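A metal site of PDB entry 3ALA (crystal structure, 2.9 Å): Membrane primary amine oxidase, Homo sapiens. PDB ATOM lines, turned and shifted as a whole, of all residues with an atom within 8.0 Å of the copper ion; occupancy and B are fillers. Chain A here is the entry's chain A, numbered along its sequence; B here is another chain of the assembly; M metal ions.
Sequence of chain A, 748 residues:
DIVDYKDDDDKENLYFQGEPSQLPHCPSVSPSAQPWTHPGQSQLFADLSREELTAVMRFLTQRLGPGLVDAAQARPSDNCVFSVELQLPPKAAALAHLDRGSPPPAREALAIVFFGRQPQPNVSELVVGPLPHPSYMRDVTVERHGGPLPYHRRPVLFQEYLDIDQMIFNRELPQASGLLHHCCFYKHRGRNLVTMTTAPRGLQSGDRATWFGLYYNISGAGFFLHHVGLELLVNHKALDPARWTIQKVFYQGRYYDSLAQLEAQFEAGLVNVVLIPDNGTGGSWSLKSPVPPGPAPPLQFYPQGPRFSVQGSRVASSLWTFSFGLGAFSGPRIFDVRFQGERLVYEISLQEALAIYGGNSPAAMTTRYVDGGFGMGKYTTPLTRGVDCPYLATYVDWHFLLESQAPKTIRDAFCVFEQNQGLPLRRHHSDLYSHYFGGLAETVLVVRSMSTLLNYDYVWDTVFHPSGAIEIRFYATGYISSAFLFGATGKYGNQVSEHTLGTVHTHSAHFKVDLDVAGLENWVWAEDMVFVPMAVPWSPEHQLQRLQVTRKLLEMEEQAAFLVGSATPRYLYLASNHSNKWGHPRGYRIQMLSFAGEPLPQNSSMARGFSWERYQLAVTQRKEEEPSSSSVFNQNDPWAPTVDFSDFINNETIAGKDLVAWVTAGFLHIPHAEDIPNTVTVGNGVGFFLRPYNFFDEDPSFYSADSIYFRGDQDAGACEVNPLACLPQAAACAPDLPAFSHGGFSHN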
ATOM      1  N   ALA A 355      -4.150   0.550  13.809  1.00  0.00           N
ATOM      2  CA  ALA A 355      -4.016   1.098  12.469  1.00  0.00           C
ATOM      3  C   ALA A 355      -3.229   2.400  12.546  1.00  0.00           C
ATOM      4  O   ALA A 355      -3.667   3.372  13.133  1.00  0.00           O
ATOM      5  CB  ALA A 355      -5.368   1.299  11.825  1.00  0.00           C
ATOM      6  N   TYR A 357      -1.330   5.459  10.470  1.00  0.00           N
ATOM      7  CA  TYR A 357      -1.562   6.130   9.191  1.00  0.00           C
ATOM      8  C   TYR A 357      -0.443   7.088   8.839  1.00  0.00           C
ATOM      9  O   TYR A 357       0.319   7.512   9.692  1.00  0.00           O
ATOM     10  CB  TYR A 357      -2.891   6.896   9.225  1.00  0.00           C
ATOM     11  CG  TYR A 357      -4.109   6.058   8.905  1.00  0.00           C
ATOM     12  CD1 TYR A 357      -4.790   5.384   9.880  1.00  0.00           C
ATOM     13  CD2 TYR A 357      -4.581   5.958   7.615  1.00  0.00           C
ATOM     14  CE1 TYR A 357      -5.891   4.624   9.575  1.00  0.00           C
ATOM     15  CE2 TYR A 357      -5.690   5.209   7.314  1.00  0.00           C
ATOM     16  CZ  TYR A 357      -6.326   4.537   8.298  1.00  0.00           C
ATOM     17  OH  TYR A 357      -7.406   3.772   8.024  1.00  0.00           O
ATOM     18  N   ASN A 455     -14.749   3.238   9.139  1.00  0.00           N
ATOM     19  CA  ASN A 455     -14.709   2.705   7.780  1.00  0.00           C
ATOM     20  C   ASN A 455     -14.379   1.202   7.689  1.00  0.00           C
ATOM     21  O   ASN A 455     -15.019   0.525   6.928  1.00  0.00           O
ATOM     22  CB  ASN A 455     -13.703   3.518   6.967  1.00  0.00           C
ATOM     23  CG  ASN A 455     -12.456   3.795   7.759  1.00  0.00           C
ATOM     24  OD1 ASN A 455     -12.523   4.367   8.849  1.00  0.00           O
ATOM     25  ND2 ASN A 455     -11.322   3.321   7.271  1.00  0.00           N
ATOM     26  N   TPQ A 456     -13.407   0.664   8.444  1.00  0.00           N
ATOM     27  CA  TPQ A 456     -13.000  -0.747   8.246  1.00  0.00           C
ATOM     28  CB  TPQ A 456     -11.679  -1.217   8.898  1.00  0.00           C
ATOM     29  C   TPQ A 456     -14.012  -1.683   8.831  1.00  0.00           C
ATOM     30  O   TPQ A 456     -14.538  -1.436   9.889  1.00  0.00           O
ATOM     31  C1  TPQ A 456     -10.836  -0.170   9.556  1.00  0.00           C
ATOM     32  C2  TPQ A 456      -9.907   0.499   8.665  1.00  0.00           C
ATOM     33  O2  TPQ A 456      -9.882   0.153   7.460  1.00  0.00           O
ATOM     34  C3  TPQ A 456      -9.032   1.552   9.191  1.00  0.00           C
ATOM     35  C4  TPQ A 456      -9.112   1.888  10.519  1.00  0.00           C
ATOM     36  O4  TPQ A 456      -8.373   2.786  10.953  1.00  0.00           O
ATOM     37  C5  TPQ A 456     -10.036   1.192  11.422  1.00  0.00           C
ATOM     38  O5  TPQ A 456     -10.071   1.519  12.631  1.00  0.00           O
ATOM     39  C6  TPQ A 456     -10.911   0.132  10.889  1.00  0.00           C
ATOM     40  N   TYR A 458     -13.517  -5.471  10.129  1.00  0.00           N
ATOM     41  CA  TYR A 458     -12.543  -6.496  10.421  1.00  0.00           C
ATOM     42  C   TYR A 458     -13.274  -7.808  10.486  1.00  0.00           C
ATOM     43  O   TYR A 458     -14.347  -7.881  11.087  1.00  0.00           O
ATOM     44  CB  TYR A 458     -11.873  -6.212  11.771  1.00  0.00           C
ATOM     45  CG  TYR A 458     -10.901  -5.016  11.756  1.00  0.00           C
ATOM     46  CD1 TYR A 458      -9.869  -4.964  10.848  1.00  0.00           C
ATOM     47  CD2 TYR A 458     -11.010  -3.992  12.656  1.00  0.00           C
ATOM     48  CE1 TYR A 458      -8.978  -3.895  10.820  1.00  0.00           C
ATOM     49  CE2 TYR A 458     -10.126  -2.931  12.664  1.00  0.00           C
ATOM     50  CZ  TYR A 458      -9.112  -2.877  11.742  1.00  0.00           C
ATOM     51  OH  TYR A 458      -8.218  -1.817  11.723  1.00  0.00           O
ATOM     52  N   ALA A 476      -9.155  -7.521   6.820  1.00  0.00           N
ATOM     53  CA  ALA A 476      -9.682  -6.155   6.849  1.00  0.00           C
ATOM     54  C   ALA A 476     -10.395  -5.917   5.545  1.00  0.00           C
ATOM     55  O   ALA A 476      -9.856  -6.176   4.470  1.00  0.00           O
ATOM     56  CB  ALA A 476      -8.572  -5.159   7.012  1.00  0.00           C
ATOM     57  N   THR A 477     -11.618  -5.433   5.645  1.00  0.00           N
ATOM     58  CA  THR A 477     -12.387  -5.050   4.484  1.00  0.00           C
ATOM     59  C   THR A 477     -13.125  -3.776   4.835  1.00  0.00           C
ATOM     60  O   THR A 477     -12.815  -3.125   5.823  1.00  0.00           O
ATOM     61  CB  THR A 477     -13.345  -6.176   4.046  1.00  0.00           C
ATOM     62  OG1 THR A 477     -14.032  -5.803   2.848  1.00  0.00           O
ATOM     63  CG2 THR A 477     -14.340  -6.489   5.130  1.00  0.00           C
ATOM     64  N   GLY A 478     -14.083  -3.416   3.999  1.00  0.00           N
ATOM     65  CA  GLY A 478     -14.836  -2.211   4.183  1.00  0.00           C
ATOM     66  C   GLY A 478     -14.187  -1.075   3.420  1.00  0.00           C
ATOM     67  O   GLY A 478     -13.469  -1.275   2.414  1.00  0.00           O
ATOM     68  N   TYR A 479     -14.456   0.127   3.902  1.00  0.00           N
ATOM     69  CA  TYR A 479     -14.078   1.320   3.203  1.00  0.00           C
ATOM     70  C   TYR A 479     -12.682   1.657   3.638  1.00  0.00           C
ATOM     71  O   TYR A 479     -12.331   1.391   4.773  1.00  0.00           O
ATOM     72  CB  TYR A 479     -15.071   2.441   3.524  1.00  0.00           C
ATOM     73  CG  TYR A 479     -16.220   2.537   2.538  1.00  0.00           C
ATOM     74  CD1 TYR A 479     -17.496   2.093   2.857  1.00  0.00           C
ATOM     75  CD2 TYR A 479     -16.017   3.090   1.299  1.00  0.00           C
ATOM     76  CE1 TYR A 479     -18.520   2.203   1.931  1.00  0.00           C
ATOM     77  CE2 TYR A 479     -17.021   3.174   0.382  1.00  0.00           C
ATOM     78  CZ  TYR A 479     -18.265   2.732   0.682  1.00  0.00           C
ATOM     79  OH  TYR A 479     -19.211   2.868  -0.315  1.00  0.00           O
ATOM     80  N   ILE A 480     -11.878   2.205   2.731  1.00  0.00           N
ATOM     81  CA  ILE A 480     -10.641   2.839   3.132  1.00  0.00           C
ATOM     82  C   ILE A 480     -10.970   4.196   3.664  1.00  0.00           C
ATOM     83  O   ILE A 480     -12.039   4.713   3.418  1.00  0.00           O
ATOM     84  CB  ILE A 480      -9.580   3.002   1.993  1.00  0.00           C
ATOM     85  CG1 ILE A 480     -10.099   3.891   0.873  1.00  0.00           C
ATOM     86  CG2 ILE A 480      -9.136   1.694   1.446  1.00  0.00           C
ATOM     87  CD1 ILE A 480      -9.045   4.626   0.227  1.00  0.00           C
ATOM     88  N   SER A 481     -10.029   4.778   4.383  1.00  0.00           N
ATOM     89  CA  SER A 481     -10.126   6.144   4.849  1.00  0.00           C
ATOM     90  C   SER A 481      -9.394   7.024   3.855  1.00  0.00           C
ATOM     91  O   SER A 481      -8.319   6.688   3.420  1.00  0.00           O
ATOM     92  CB  SER A 481      -9.507   6.254   6.229  1.00  0.00           C
ATOM     93  OG  SER A 481      -8.930   7.519   6.398  1.00  0.00           O
ATOM     94  N   THR A 503      -5.107   6.977   1.813  1.00  0.00           N
ATOM     95  CA  THR A 503      -3.964   7.199   2.706  1.00  0.00           C
ATOM     96  C   THR A 503      -3.315   5.893   3.163  1.00  0.00           C
ATOM     97  O   THR A 503      -3.995   4.983   3.604  1.00  0.00           O
ATOM     98  CB  THR A 503      -4.347   8.038   3.911  1.00  0.00           C
ATOM     99  OG1 THR A 503      -5.581   7.555   4.429  1.00  0.00           O
ATOM    100  CG2 THR A 503      -4.521   9.503   3.504  1.00  0.00           C
ATOM    101  N   VAL A 504      -1.997   5.840   3.008  1.00  0.00           N
ATOM    102  CA  VAL A 504      -1.206   4.695   3.399  1.00  0.00           C
ATOM    103  C   VAL A 504      -1.374   4.447   4.872  1.00  0.00           C
ATOM    104  O   VAL A 504      -1.554   5.361   5.633  1.00  0.00           O
ATOM    105  CB  VAL A 504       0.260   4.916   3.098  1.00  0.00           C
ATOM    106  CG1 VAL A 504       0.761   6.101   3.803  1.00  0.00           C
ATOM    107  CG2 VAL A 504       1.049   3.729   3.530  1.00  0.00           C
ATOM    108  N   HIS A 505      -1.331   3.184   5.262  1.00  0.00           N
ATOM    109  CA  HIS A 505      -1.403   2.806   6.658  1.00  0.00           C
ATOM    110  C   HIS A 505      -1.054   1.315   6.830  1.00  0.00           C
ATOM    111  O   HIS A 505      -0.958   0.592   5.866  1.00  0.00           O
ATOM    112  CB  HIS A 505      -2.797   3.022   7.175  1.00  0.00           C
ATOM    113  CG  HIS A 505      -3.805   2.272   6.413  1.00  0.00           C
ATOM    114  ND1 HIS A 505      -4.177   2.631   5.150  1.00  0.00           N
ATOM    115  CD2 HIS A 505      -4.486   1.142   6.702  1.00  0.00           C
ATOM    116  CE1 HIS A 505      -5.069   1.766   4.695  1.00  0.00           C
ATOM    117  NE2 HIS A 505      -5.252   0.852   5.612  1.00  0.00           N
ATOM    118  N   THR A 506      -0.881   0.901   8.076  1.00  0.00           N
ATOM    119  CA  THR A 506      -0.639  -0.493   8.398  1.00  0.00           C
ATOM    120  C   THR A 506      -1.713  -0.990   9.330  1.00  0.00           C
ATOM    121  O   THR A 506      -2.168  -0.261  10.161  1.00  0.00           O
ATOM    122  CB  THR A 506       0.660  -0.683   9.158  1.00  0.00           C
ATOM    123  OG1 THR A 506       0.576   0.023  10.398  1.00  0.00           O
ATOM    124  CG2 THR A 506       1.825  -0.172   8.372  1.00  0.00           C
ATOM    125  N   HIS A 507      -2.083  -2.251   9.184  1.00  0.00           N
ATOM    126  CA  HIS A 507      -2.952  -2.928  10.121  1.00  0.00           C
ATOM    127  C   HIS A 507      -2.128  -3.888  10.927  1.00  0.00           C
ATOM    128  O   HIS A 507      -1.162  -4.424  10.427  1.00  0.00           O
ATOM    129  CB  HIS A 507      -4.018  -3.741   9.395  1.00  0.00           C
ATOM    130  CG  HIS A 507      -5.021  -2.903   8.675  1.00  0.00           C
ATOM    131  ND1 HIS A 507      -6.168  -2.434   9.279  1.00  0.00           N
ATOM    132  CD2 HIS A 507      -5.047  -2.436   7.396  1.00  0.00           C
ATOM    133  CE1 HIS A 507      -6.845  -1.700   8.414  1.00  0.00           C
ATOM    134  NE2 HIS A 507      -6.193  -1.692   7.272  1.00  0.00           N
ATOM    135  N   PHE A 667      -0.034  -6.180   8.382  1.00  0.00           N
ATOM    136  CA  PHE A 667       0.476  -5.886   7.061  1.00  0.00           C
ATOM    137  C   PHE A 667       0.349  -4.401   6.715  1.00  0.00           C
ATOM    138  O   PHE A 667      -0.413  -3.653   7.357  1.00  0.00           O
ATOM    139  CB  PHE A 667      -0.284  -6.682   6.008  1.00  0.00           C
ATOM    140  CG  PHE A 667      -1.738  -6.401   5.985  1.00  0.00           C
ATOM    141  CD1 PHE A 667      -2.270  -5.524   5.058  1.00  0.00           C
ATOM    142  CD2 PHE A 667      -2.593  -7.017   6.877  1.00  0.00           C
ATOM    143  CE1 PHE A 667      -3.637  -5.236   5.035  1.00  0.00           C
ATOM    144  CE2 PHE A 667      -3.971  -6.741   6.866  1.00  0.00           C
ATOM    145  CZ  PHE A 667      -4.492  -5.846   5.934  1.00  0.00           C
ATOM    146  N   LEU A 668       1.096  -3.988   5.692  1.00  0.00           N
ATOM    147  CA  LEU A 668       1.077  -2.631   5.183  1.00  0.00           C
ATOM    148  C   LEU A 668       0.055  -2.520   4.077  1.00  0.00           C
ATOM    149  O   LEU A 668      -0.048  -3.374   3.238  1.00  0.00           O
ATOM    150  CB  LEU A 668       2.442  -2.260   4.638  1.00  0.00           C
ATOM    151  CG  LEU A 668       2.499  -1.031   3.721  1.00  0.00           C
ATOM    152  CD1 LEU A 668       2.157   0.240   4.473  1.00  0.00           C
ATOM    153  CD2 LEU A 668       3.839  -0.908   3.108  1.00  0.00           C
ATOM    154  N   HIS A 669      -0.706  -1.441   4.063  1.00  0.00           N
ATOM    155  CA  HIS A 669      -1.672  -1.220   3.015  1.00  0.00           C
ATOM    156  C   HIS A 669      -1.440   0.135   2.379  1.00  0.00           C
ATOM    157  O   HIS A 669      -1.579   1.143   3.035  1.00  0.00           O
ATOM    158  CB  HIS A 669      -3.090  -1.319   3.582  1.00  0.00           C
ATOM    159  CG  HIS A 669      -4.170  -1.266   2.549  1.00  0.00           C
ATOM    160  ND1 HIS A 669      -5.507  -1.206   2.878  1.00  0.00           N
ATOM    161  CD2 HIS A 669      -4.119  -1.219   1.206  1.00  0.00           C
ATOM    162  CE1 HIS A 669      -6.223  -1.136   1.789  1.00  0.00           C
ATOM    163  NE2 HIS A 669      -5.404  -1.137   0.753  1.00  0.00           N
ATOM    164  N   ILE A 670      -1.047   0.126   1.120  1.00  0.00           N
ATOM    165  CA  ILE A 670      -0.990   1.307   0.289  1.00  0.00           C
ATOM    166  C   ILE A 670      -2.218   1.250  -0.602  1.00  0.00           C
ATOM    167  O   ILE A 670      -2.300   0.441  -1.526  1.00  0.00           O
ATOM    168  CB  ILE A 670       0.187   1.286  -0.630  1.00  0.00           C
ATOM    169  CG1 ILE A 670       1.484   1.198   0.145  1.00  0.00           C
ATOM    170  CG2 ILE A 670       0.164   2.513  -1.471  1.00  0.00           C
ATOM    171  CD1 ILE A 670       2.721   1.083  -0.745  1.00  0.00           C
ATOM    172  N   PRO A 671      -3.222   2.099  -0.326  1.00  0.00           N
ATOM    173  CA  PRO A 671      -4.421   1.971  -1.111  1.00  0.00           C
ATOM    174  C   PRO A 671      -4.226   2.216  -2.596  1.00  0.00           C
ATOM    175  O   PRO A 671      -3.309   2.920  -2.996  1.00  0.00           O
ATOM    176  CB  PRO A 671      -5.314   3.026  -0.500  1.00  0.00           C
ATOM    177  CG  PRO A 671      -4.891   3.084   0.888  1.00  0.00           C
ATOM    178  CD  PRO A 671      -3.434   2.965   0.841  1.00  0.00           C
ATOM    179  N   ASP A 675      -9.271  -0.753  -4.235  1.00  0.00           N
ATOM    180  CA  ASP A 675      -9.914  -0.586  -2.928  1.00  0.00           C
ATOM    181  C   ASP A 675     -11.206   0.247  -2.961  1.00  0.00           C
ATOM    182  O   ASP A 675     -11.790   0.493  -1.939  1.00  0.00           O
ATOM    183  CB  ASP A 675      -8.927   0.041  -1.939  1.00  0.00           C
ATOM    184  CG  ASP A 675      -7.729  -0.842  -1.673  1.00  0.00           C
ATOM    185  OD1 ASP A 675      -7.866  -2.038  -1.345  1.00  0.00           O
ATOM    186  OD2 ASP A 675      -6.611  -0.337  -1.789  1.00  0.00           O
ATOM    187  N   THR A 679     -12.232  -2.423   0.117  1.00  0.00           N
ATOM    188  CA  THR A 679     -11.073  -3.292   0.111  1.00  0.00           C
ATOM    189  C   THR A 679     -11.549  -4.724   0.135  1.00  0.00           C
ATOM    190  O   THR A 679     -12.378  -5.081   0.958  1.00  0.00           O
ATOM    191  CB  THR A 679     -10.223  -3.081   1.366  1.00  0.00           C
ATOM    192  OG1 THR A 679      -9.797  -1.725   1.405  1.00  0.00           O
ATOM    193  CG2 THR A 679      -9.005  -3.987   1.377  1.00  0.00           C
ATOM    194  N   ASN A 684      -5.497 -10.645   1.766  1.00  0.00           N
ATOM    195  CA  ASN A 684      -5.298  -9.799   2.949  1.00  0.00           C
ATOM    196  C   ASN A 684      -5.569 -10.486   4.279  1.00  0.00           C
ATOM    197  O   ASN A 684      -5.519  -9.845   5.309  1.00  0.00           O
ATOM    198  CB  ASN A 684      -6.181  -8.540   2.871  1.00  0.00           C
ATOM    199  CG  ASN A 684      -5.726  -7.586   1.771  1.00  0.00           C
ATOM    200  OD1 ASN A 684      -4.513  -7.408   1.516  1.00  0.00           O
ATOM    201  ND2 ASN A 684      -6.699  -6.954   1.107  1.00  0.00           N
ATOM    202  N   TYR B 571       5.826  -4.234  -1.525  1.00  0.00           N
ATOM    203  CA  TYR B 571       4.980  -4.181  -2.698  1.00  0.00           C
ATOM    204  C   TYR B 571       5.891  -4.288  -3.889  1.00  0.00           C
ATOM    205  O   TYR B 571       6.735  -3.446  -4.084  1.00  0.00           O
ATOM    206  CB  TYR B 571       4.235  -2.854  -2.769  1.00  0.00           C
ATOM    207  CG  TYR B 571       2.914  -2.815  -2.063  1.00  0.00           C
ATOM    208  CD1 TYR B 571       2.823  -2.887  -0.680  1.00  0.00           C
ATOM    209  CD2 TYR B 571       1.747  -2.670  -2.764  1.00  0.00           C
ATOM    210  CE1 TYR B 571       1.613  -2.839  -0.032  1.00  0.00           C
ATOM    211  CE2 TYR B 571       0.529  -2.617  -2.119  1.00  0.00           C
ATOM    212  CZ  TYR B 571       0.478  -2.698  -0.759  1.00  0.00           C
ATOM    213  OH  TYR B 571      -0.697  -2.660  -0.090  1.00  0.00           O
HETATM  214 CU    CU M   1      -6.064  -0.989   5.013  1.00  0.00          CU
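The side-chain carboxylate of Asp 675 is in hydrogen-bond range of a ring nitrogen (NE2) of His 669, 2.9 Å away. OH of Tyr 458 is in hydrogen-bond range of ND1 of His 507 (3.2 Å). The backbone carbonyl oxygen (O) of Thr 503 is in hydrogen-bond range of a ring nitrogen (ND1) of His 505 (2.8 Å). The backbone NH (N) of His 507 lies within hydrogen-bond range of the backbone carbonyl oxygen (O) of Phe 667, at 2.8 Å.
The copper ion is bound by NE2 of His 505, ND1 of His 669 and NE2 of His 507. The copper ion has three donor atoms within binding distance.
The nearest printed residue that does not touch the copper ion is TPQ 456 (4.7 Å).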
